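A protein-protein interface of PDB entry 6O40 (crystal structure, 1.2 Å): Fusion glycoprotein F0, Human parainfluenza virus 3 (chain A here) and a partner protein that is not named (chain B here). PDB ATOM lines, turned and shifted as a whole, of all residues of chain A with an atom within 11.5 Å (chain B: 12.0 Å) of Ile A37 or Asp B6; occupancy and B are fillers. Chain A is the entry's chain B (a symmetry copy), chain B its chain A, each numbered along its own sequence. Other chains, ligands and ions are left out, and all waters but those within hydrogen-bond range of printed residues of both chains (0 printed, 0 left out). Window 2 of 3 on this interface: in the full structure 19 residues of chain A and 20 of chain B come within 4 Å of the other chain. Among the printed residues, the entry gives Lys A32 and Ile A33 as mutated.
Arg A29 touches Asp B16. N of Ser A30 touches OD2 of Asp B16, 3.7 Å away. Lys B9 touches Ile A33 (O to CG2, 3.2 Å). Ile A33 touches Glu B12. OD2 of Asp B16 touches CD1 of Ile A33 (3.3 Å). Leu A34 touches Ala B13 (CD2 to CB, 3.5 Å). Lys B9 touches Ile A37 (CB to CG1, 3.8 Å). Leu B10 touches Ile A37.
Ile A37 touches three residues of chain B. Asp B6 touches just one residue of chain A: Ile A37 (3.2 Å). Ser A36 touches just one residue of chain B: Lys B9 (3.0 Å). No residue of chain B comes within 4 Å of NH2 A38. No residue of chain A comes within 4 Å of Ala B3. No residue of chain A comes within 4 Å of Ser B5. No residue of chain A comes within 4 Å of Ile B7. Of the printed residues of chain A, Lys B9 touches Ile A33, Ser A36 and Ile A37. Of chain A, only Ile A37 comes within 4 Å of Leu B10. Of the printed residues of chain A, Thr B17 touches Ser A30. Of the printed residues of chain B, Ser A30 touches Ala B13, Asp B16 and Thr B17. Of the printed residues of chain A, Glu B12 touches Ile A33 (3.95 Å). Lys B11 touches none of the printed residues of chain A. Asn A31 touches none of the printed residues of chain B. The nearest residue of chain B that does not touch Ile A37 is Ala B13 (5.9 Å). The nearest residue of chain A that does not touch Asp B6 is Ser A36 (5.0 Å).
Printed residues of chain B that touch a printed residue of chain A: Asp B6, Lys B9, Leu B10, Glu B12, Ala B13, Asp B16 and Thr B17. Hydrophobic or aromatic side chains of chain B that line the printed part of chain A: Leu B10 and Ala B13. Hydrophobic or aromatic side chains of chain A that line the printed part of chain B: Ile A33, Leu A34 and Ile A37. Among the printed residues, 12 pairs touch across the chains. Among the printed residues, no Asp or Glu carboxylate lies within 4 Å of a Lys or Arg side-chain nitrogen of the other chain.
The side-chain hydroxyl (OG) of Ser A30 sits at hydrogen-bond distance from the backbone carbonyl oxygen (O) of Ala B13. O of Ser A36 lies within hydrogen-bond range of NZ of Lys B9 (3.0 Å). O of Ile A37 sits close to OD1 of Asp B6, 3.2 Å away. OG1 of Thr B17 sits at hydrogen-bond distance from OG of Ser A30.
O of Ala B13 is in hydrogen-bond range of OG1 of Thr B17, at 3.1 Å. O of Ile A33 sits at hydrogen-bond distance from OG of Ser A36 (2.6 Å). The side-chain carboxylate (OE2) of Glu B12 is in salt-bridge range of the guanidinium group (NH1) of Arg B15 (2.9 Å).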
ATOM      1  N   ARG A  29     -24.946 -19.003   3.625  1.00  0.00           N
ATOM      2  CA  ARG A  29     -24.609 -19.932   2.560  1.00  0.00           C
ATOM      3  C   ARG A  29     -23.298 -20.653   2.838  1.00  0.00           C
ATOM      4  O   ARG A  29     -23.179 -21.852   2.549  1.00  0.00           O
ATOM      5  CB  ARG A  29     -24.599 -19.183   1.235  1.00  0.00           C
ATOM      6  CG  ARG A  29     -25.992 -18.709   0.882  1.00  0.00           C
ATOM      7  CD  ARG A  29     -26.109 -18.153  -0.489  1.00  0.00           C
ATOM      8  NE  ARG A  29     -27.484 -17.733  -0.756  1.00  0.00           N
ATOM      9  CZ  ARG A  29     -28.106 -17.863  -1.920  1.00  0.00           C
ATOM     10  NH1 ARG A  29     -27.499 -18.437  -2.941  1.00  0.00           N
ATOM     11  NH2 ARG A  29     -29.351 -17.429  -2.061  1.00  0.00           N
ATOM     12  N   SER A  30     -22.290 -19.957   3.374  1.00  0.00           N
ATOM     13  CA  SER A  30     -21.035 -20.613   3.731  1.00  0.00           C
ATOM     14  C   SER A  30     -21.280 -21.708   4.756  1.00  0.00           C
ATOM     15  O   SER A  30     -20.817 -22.848   4.599  1.00  0.00           O
ATOM     16  CB  SER A  30     -20.077 -19.563   4.311  1.00  0.00           C
ATOM     17  OG  SER A  30     -18.870 -20.190   4.723  1.00  0.00           O
ATOM     18  N   ASN A  31     -22.053 -21.397   5.790  1.00  0.00           N
ATOM     19  CA  ASN A  31     -22.369 -22.357   6.878  1.00  0.00           C
ATOM     20  C   ASN A  31     -23.124 -23.563   6.304  1.00  0.00           C
ATOM     21  O   ASN A  31     -22.837 -24.678   6.730  1.00  0.00           O
ATOM     22  CB  ASN A  31     -23.143 -21.684   8.011  1.00  0.00           C
ATOM     23  CG  ASN A  31     -22.248 -20.885   8.932  1.00  0.00           C
ATOM     24  OD1 ASN A  31     -21.079 -21.205   9.100  1.00  0.00           O
ATOM     25  ND2 ASN A  31     -22.794 -19.843   9.526  1.00  0.00           N
ATOM     26  N   LYS A  32     -24.037 -23.347   5.362  1.00  0.00           N
ATOM     27  CA  LYS A  32     -24.824 -24.442   4.742  1.00  0.00           C
ATOM     28  C   LYS A  32     -23.873 -25.374   3.984  1.00  0.00           C
ATOM     29  O   LYS A  32     -24.027 -26.587   4.102  1.00  0.00           O
ATOM     30  CB  LYS A  32     -25.916 -23.885   3.829  1.00  0.00           C
ATOM     31  CG  LYS A  32     -26.830 -24.937   3.220  1.00  0.00           C
ATOM     32  CD  LYS A  32     -27.908 -24.372   2.333  1.00  0.00           C
ATOM     33  CE  LYS A  32     -28.773 -25.449   1.712  1.00  0.00           C
ATOM     34  NZ  LYS A  32     -30.084 -24.919   1.277  1.00  0.00           N
ATOM     35  N   ILE A  33     -22.919 -24.827   3.231  1.00  0.00           N
ATOM     36  CA  ILE A  33     -21.944 -25.659   2.470  1.00  0.00           C
ATOM     37  C   ILE A  33     -21.111 -26.472   3.466  1.00  0.00           C
ATOM     38  O   ILE A  33     -20.882 -27.652   3.205  1.00  0.00           O
ATOM     39  CB  ILE A  33     -21.057 -24.813   1.545  1.00  0.00           C
ATOM     40  CG1 ILE A  33     -21.871 -24.185   0.413  1.00  0.00           C
ATOM     41  CG2 ILE A  33     -19.907 -25.654   1.017  1.00  0.00           C
ATOM     42  CD1 ILE A  33     -21.125 -23.143  -0.373  1.00  0.00           C
ATOM     43  N   LEU A  34     -20.661 -25.865   4.564  1.00  0.00           N
ATOM     44  CA  LEU A  34     -19.826 -26.556   5.584  1.00  0.00           C
ATOM     45  C   LEU A  34     -20.614 -27.725   6.175  1.00  0.00           C
ATOM     46  O   LEU A  34     -20.030 -28.785   6.385  1.00  0.00           O
ATOM     47  CB  LEU A  34     -19.405 -25.574   6.677  1.00  0.00           C
ATOM     48  CG  LEU A  34     -18.442 -24.478   6.234  1.00  0.00           C
ATOM     49  CD1 LEU A  34     -18.157 -23.525   7.384  1.00  0.00           C
ATOM     50  CD2 LEU A  34     -17.157 -25.068   5.676  1.00  0.00           C
ATOM     51  N   ASP A  35     -21.927 -27.559   6.348  1.00  0.00           N
ATOM     52  CA  ASP A  35     -22.835 -28.591   6.917  1.00  0.00           C
ATOM     53  C   ASP A  35     -22.910 -29.813   5.986  1.00  0.00           C
ATOM     54  O   ASP A  35     -23.171 -30.909   6.497  1.00  0.00           O
ATOM     55  CB  ASP A  35     -24.231 -28.013   7.178  1.00  0.00           C
ATOM     56  CG  ASP A  35     -24.314 -27.075   8.370  1.00  0.00           C
ATOM     57  OD1 ASP A  35     -23.325 -26.966   9.104  1.00  0.00           O
ATOM     58  OD2 ASP A  35     -25.370 -26.456   8.550  1.00  0.00           O
ATOM     59  N   SER A  36     -22.714 -29.636   4.677  1.00  0.00           N
ATOM     60  CA  SER A  36     -22.777 -30.708   3.654  1.00  0.00           C
ATOM     61  C   SER A  36     -21.471 -31.508   3.559  1.00  0.00           C
ATOM     62  O   SER A  36     -21.465 -32.470   2.791  1.00  0.00           O
ATOM     63  CB  SER A  36     -23.132 -30.126   2.315  1.00  0.00           C
ATOM     64  OG  SER A  36     -22.012 -29.493   1.717  1.00  0.00           O
ATOM     65  N   ILE A  37     -20.411 -31.168   4.299  1.00  0.00           N
ATOM     66  CA  ILE A  37     -19.133 -31.857   4.169  1.00  0.00           C
ATOM     67  C   ILE A  37     -19.194 -33.220   4.827  1.00  0.00           C
ATOM     68  O   ILE A  37     -18.661 -34.200   4.302  1.00  0.00           O
ATOM     69  CB  ILE A  37     -17.985 -30.994   4.721  1.00  0.00           C
ATOM     70  CG1 ILE A  37     -17.697 -29.867   3.711  1.00  0.00           C
ATOM     71  CG2 ILE A  37     -16.768 -31.834   5.067  1.00  0.00           C
ATOM     72  CD1 ILE A  37     -16.811 -28.763   4.199  1.00  0.00           C
ATOM     73  N   NH2 A  38     -19.857 -33.279   5.974  1.00  0.00           N
ATOM     74  N   ALA B   3     -11.368 -37.284  -1.689  1.00  0.00           N
ATOM     75  CA  ALA B   3     -11.639 -36.079  -0.914  1.00  0.00           C
ATOM     76  C   ALA B   3     -11.787 -34.855  -1.812  1.00  0.00           C
ATOM     77  O   ALA B   3     -11.872 -33.717  -1.328  1.00  0.00           O
ATOM     78  CB  ALA B   3     -10.537 -35.852   0.098  1.00  0.00           C
ATOM     79  N   ARG B   4     -11.822 -35.071  -3.125  1.00  0.00           N
ATOM     80  CA  ARG B   4     -11.979 -33.950  -4.049  1.00  0.00           C
ATOM     81  C   ARG B   4     -13.284 -33.193  -3.785  1.00  0.00           C
ATOM     82  O   ARG B   4     -13.300 -31.955  -3.773  1.00  0.00           O
ATOM     83  CB  ARG B   4     -11.896 -34.443  -5.497  1.00  0.00           C
ATOM     84  CG  ARG B   4     -11.964 -33.338  -6.545  1.00  0.00           C
ATOM     85  CD  ARG B   4     -12.645 -33.832  -7.821  1.00  0.00           C
ATOM     86  NE  ARG B   4     -13.938 -34.385  -7.442  1.00  0.00           N
ATOM     87  CZ  ARG B   4     -15.040 -33.662  -7.261  1.00  0.00           C
ATOM     88  NH1 ARG B   4     -15.040 -32.349  -7.481  1.00  0.00           N
ATOM     89  NH2 ARG B   4     -16.148 -34.263  -6.874  1.00  0.00           N
ATOM     90  N   SER B   5     -14.371 -33.917  -3.507  1.00  0.00           N
ATOM     91  CA  SER B   5     -15.657 -33.293  -3.223  1.00  0.00           C
ATOM     92  C   SER B   5     -15.592 -32.412  -1.979  1.00  0.00           C
ATOM     93  O   SER B   5     -16.142 -31.297  -1.971  1.00  0.00           O
ATOM     94  CB  SER B   5     -16.725 -34.383  -3.061  1.00  0.00           C
ATOM     95  OG  SER B   5     -18.007 -33.814  -2.891  1.00  0.00           O
ATOM     96  N   ASP B   6     -14.937 -32.884  -0.915  1.00  0.00           N
ATOM     97  CA  ASP B   6     -14.833 -32.083   0.303  1.00  0.00           C
ATOM     98  C   ASP B   6     -13.931 -30.865   0.092  1.00  0.00           C
ATOM     99  O   ASP B   6     -14.221 -29.780   0.613  1.00  0.00           O
ATOM    100  CB  ASP B   6     -14.337 -32.930   1.473  1.00  0.00           C
ATOM    101  CG  ASP B   6     -15.425 -33.846   2.066  1.00  0.00           C
ATOM    102  OD1 ASP B   6     -16.634 -33.575   1.919  1.00  0.00           O
ATOM    103  OD2 ASP B   6     -15.052 -34.854   2.707  1.00  0.00           O
ATOM    104  N   ILE B   7     -12.867 -30.998  -0.695  1.00  0.00           N
ATOM    105  CA  ILE B   7     -11.997 -29.864  -0.992  1.00  0.00           C
ATOM    106  C   ILE B   7     -12.777 -28.807  -1.742  1.00  0.00           C
ATOM    107  O   ILE B   7     -12.666 -27.607  -1.460  1.00  0.00           O
ATOM    108  CB  ILE B   7     -10.781 -30.333  -1.812  1.00  0.00           C
ATOM    109  CG1 ILE B   7      -9.925 -31.301  -0.995  1.00  0.00           C
ATOM    110  CG2 ILE B   7      -9.985 -29.167  -2.299  1.00  0.00           C
ATOM    111  CD1 ILE B   7      -9.171 -30.702   0.104  1.00  0.00           C
ATOM    112  N   GLU B   8     -13.612 -29.228  -2.692  1.00  0.00           N
ATOM    113  CA  GLU B   8     -14.400 -28.288  -3.480  1.00  0.00           C
ATOM    114  C   GLU B   8     -15.433 -27.585  -2.616  1.00  0.00           C
ATOM    115  O   GLU B   8     -15.680 -26.389  -2.796  1.00  0.00           O
ATOM    116  CB  GLU B   8     -15.057 -29.028  -4.648  1.00  0.00           C
ATOM    117  CG  GLU B   8     -14.066 -29.400  -5.756  1.00  0.00           C
ATOM    118  CD  GLU B   8     -13.357 -28.189  -6.350  1.00  0.00           C
ATOM    119  OE1 GLU B   8     -14.052 -27.230  -6.750  1.00  0.00           O
ATOM    120  OE2 GLU B   8     -12.108 -28.188  -6.398  1.00  0.00           O
ATOM    121  N   LYS B   9     -16.021 -28.295  -1.659  1.00  0.00           N
ATOM    122  CA  LYS B   9     -16.963 -27.677  -0.735  1.00  0.00           C
ATOM    123  C   LYS B   9     -16.263 -26.644   0.144  1.00  0.00           C
ATOM    124  O   LYS B   9     -16.779 -25.546   0.371  1.00  0.00           O
ATOM    125  CB  LYS B   9     -17.641 -28.730   0.130  1.00  0.00           C
ATOM    126  CG  LYS B   9     -18.702 -29.540  -0.645  1.00  0.00           C
ATOM    127  CD  LYS B   9     -19.263 -30.695   0.160  1.00  0.00           C
ATOM    128  CE  LYS B   9     -20.363 -31.379  -0.642  1.00  0.00           C
ATOM    129  NZ  LYS B   9     -20.707 -32.715  -0.095  1.00  0.00           N
ATOM    130  N   LEU B  10     -15.097 -26.986   0.684  1.00  0.00           N
ATOM    131  CA  LEU B  10     -14.341 -26.044   1.549  1.00  0.00           C
ATOM    132  C   LEU B  10     -14.018 -24.793   0.729  1.00  0.00           C
ATOM    133  O   LEU B  10     -14.197 -23.688   1.232  1.00  0.00           O
ATOM    134  CB  LEU B  10     -13.073 -26.721   2.071  1.00  0.00           C
ATOM    135  CG  LEU B  10     -13.310 -27.765   3.159  1.00  0.00           C
ATOM    136  CD1 LEU B  10     -12.070 -28.615   3.370  1.00  0.00           C
ATOM    137  CD2 LEU B  10     -13.738 -27.109   4.459  1.00  0.00           C
ATOM    138  N   LYS B  11     -13.582 -24.977  -0.512  1.00  0.00           N
ATOM    139  CA  LYS B  11     -13.248 -23.857  -1.421  1.00  0.00           C
ATOM    140  C   LYS B  11     -14.482 -22.967  -1.587  1.00  0.00           C
ATOM    141  O   LYS B  11     -14.352 -21.752  -1.459  1.00  0.00           O
ATOM    142  CB  LYS B  11     -12.786 -24.387  -2.778  1.00  0.00           C
ATOM    143  CG  LYS B  11     -12.492 -23.316  -3.815  1.00  0.00           C
ATOM    144  CD  LYS B  11     -12.109 -23.877  -5.168  1.00  0.00           C
ATOM    145  CE  LYS B  11     -13.200 -24.731  -5.772  1.00  0.00           C
ATOM    146  NZ  LYS B  11     -12.733 -25.403  -7.006  1.00  0.00           N
ATOM    147  N   GLU B  12     -15.648 -23.555  -1.852  1.00  0.00           N
ATOM    148  CA  GLU B  12     -16.848 -22.758  -2.081  1.00  0.00           C
ATOM    149  C   GLU B  12     -17.325 -22.076  -0.807  1.00  0.00           C
ATOM    150  O   GLU B  12     -17.803 -20.932  -0.867  1.00  0.00           O
ATOM    151  CB  GLU B  12     -17.957 -23.624  -2.690  1.00  0.00           C
ATOM    152  CG  GLU B  12     -17.698 -24.003  -4.149  1.00  0.00           C
ATOM    153  CD  GLU B  12     -17.457 -22.777  -5.025  1.00  0.00           C
ATOM    154  OE1 GLU B  12     -18.264 -21.832  -4.958  1.00  0.00           O
ATOM    155  OE2 GLU B  12     -16.445 -22.738  -5.753  1.00  0.00           O
ATOM    156  N   ALA B  13     -17.171 -22.719   0.346  1.00  0.00           N
ATOM    157  CA  ALA B  13     -17.497 -22.065   1.611  1.00  0.00           C
ATOM    158  C   ALA B  13     -16.618 -20.840   1.836  1.00  0.00           C
ATOM    159  O   ALA B  13     -17.111 -19.792   2.260  1.00  0.00           O
ATOM    160  CB  ALA B  13     -17.362 -23.047   2.774  1.00  0.00           C
ATOM    161  N   ILE B  14     -15.309 -20.957   1.619  1.00  0.00           N
ATOM    162  CA  ILE B  14     -14.425 -19.807   1.811  1.00  0.00           C
ATOM    163  C   ILE B  14     -14.746 -18.722   0.799  1.00  0.00           C
ATOM    164  O   ILE B  14     -14.729 -17.544   1.137  1.00  0.00           O
ATOM    165  CB  ILE B  14     -12.938 -20.202   1.723  1.00  0.00           C
ATOM    166  CG1 ILE B  14     -12.563 -21.266   2.742  1.00  0.00           C
ATOM    167  CG2 ILE B  14     -12.038 -18.968   1.934  1.00  0.00           C
ATOM    168  CD1 ILE B  14     -11.263 -21.969   2.415  1.00  0.00           C
ATOM    169  N   ARG B  15     -15.096 -19.071  -0.435  1.00  0.00           N
ATOM    170  CA  ARG B  15     -15.533 -18.062  -1.397  1.00  0.00           C
ATOM    171  C   ARG B  15     -16.748 -17.304  -0.879  1.00  0.00           C
ATOM    172  O   ARG B  15     -16.813 -16.077  -0.999  1.00  0.00           O
ATOM    173  CB  ARG B  15     -15.824 -18.689  -2.768  1.00  0.00           C
ATOM    174  CG  ARG B  15     -14.551 -19.014  -3.568  1.00  0.00           C
ATOM    175  CD  ARG B  15     -14.839 -19.593  -4.954  1.00  0.00           C
ATOM    176  NE  ARG B  15     -13.589 -19.675  -5.706  1.00  0.00           N
ATOM    177  CZ  ARG B  15     -13.325 -20.542  -6.676  1.00  0.00           C
ATOM    178  NH1 ARG B  15     -14.221 -21.440  -7.049  1.00  0.00           N
ATOM    179  NH2 ARG B  15     -12.148 -20.482  -7.268  1.00  0.00           N
ATOM    180  N   ASP B  16     -17.697 -17.988  -0.244  1.00  0.00           N
ATOM    181  CA  ASP B  16     -18.872 -17.308   0.312  1.00  0.00           C
ATOM    182  C   ASP B  16     -18.489 -16.431   1.507  1.00  0.00           C
ATOM    183  O   ASP B  16     -18.985 -15.304   1.654  1.00  0.00           O
ATOM    184  CB  ASP B  16     -19.962 -18.315   0.704  1.00  0.00           C
ATOM    185  CG  ASP B  16     -20.693 -18.906  -0.496  1.00  0.00           C
ATOM    186  OD1 ASP B  16     -20.428 -18.480  -1.630  1.00  0.00           O
ATOM    187  OD2 ASP B  16     -21.509 -19.818  -0.259  1.00  0.00           O
ATOM    188  N   THR B  17     -17.621 -16.930   2.395  1.00  0.00           N
ATOM    189  CA  THR B  17     -17.118 -16.108   3.501  1.00  0.00           C
ATOM    190  C   THR B  17     -16.416 -14.866   2.980  1.00  0.00           C
ATOM    191  O   THR B  17     -16.601 -13.771   3.519  1.00  0.00           O
ATOM    192  CB  THR B  17     -16.175 -16.962   4.363  1.00  0.00           C
ATOM    193  OG1 THR B  17     -16.898 -18.104   4.864  1.00  0.00           O
ATOM    194  CG2 THR B  17     -15.591 -16.163   5.537  1.00  0.00           C
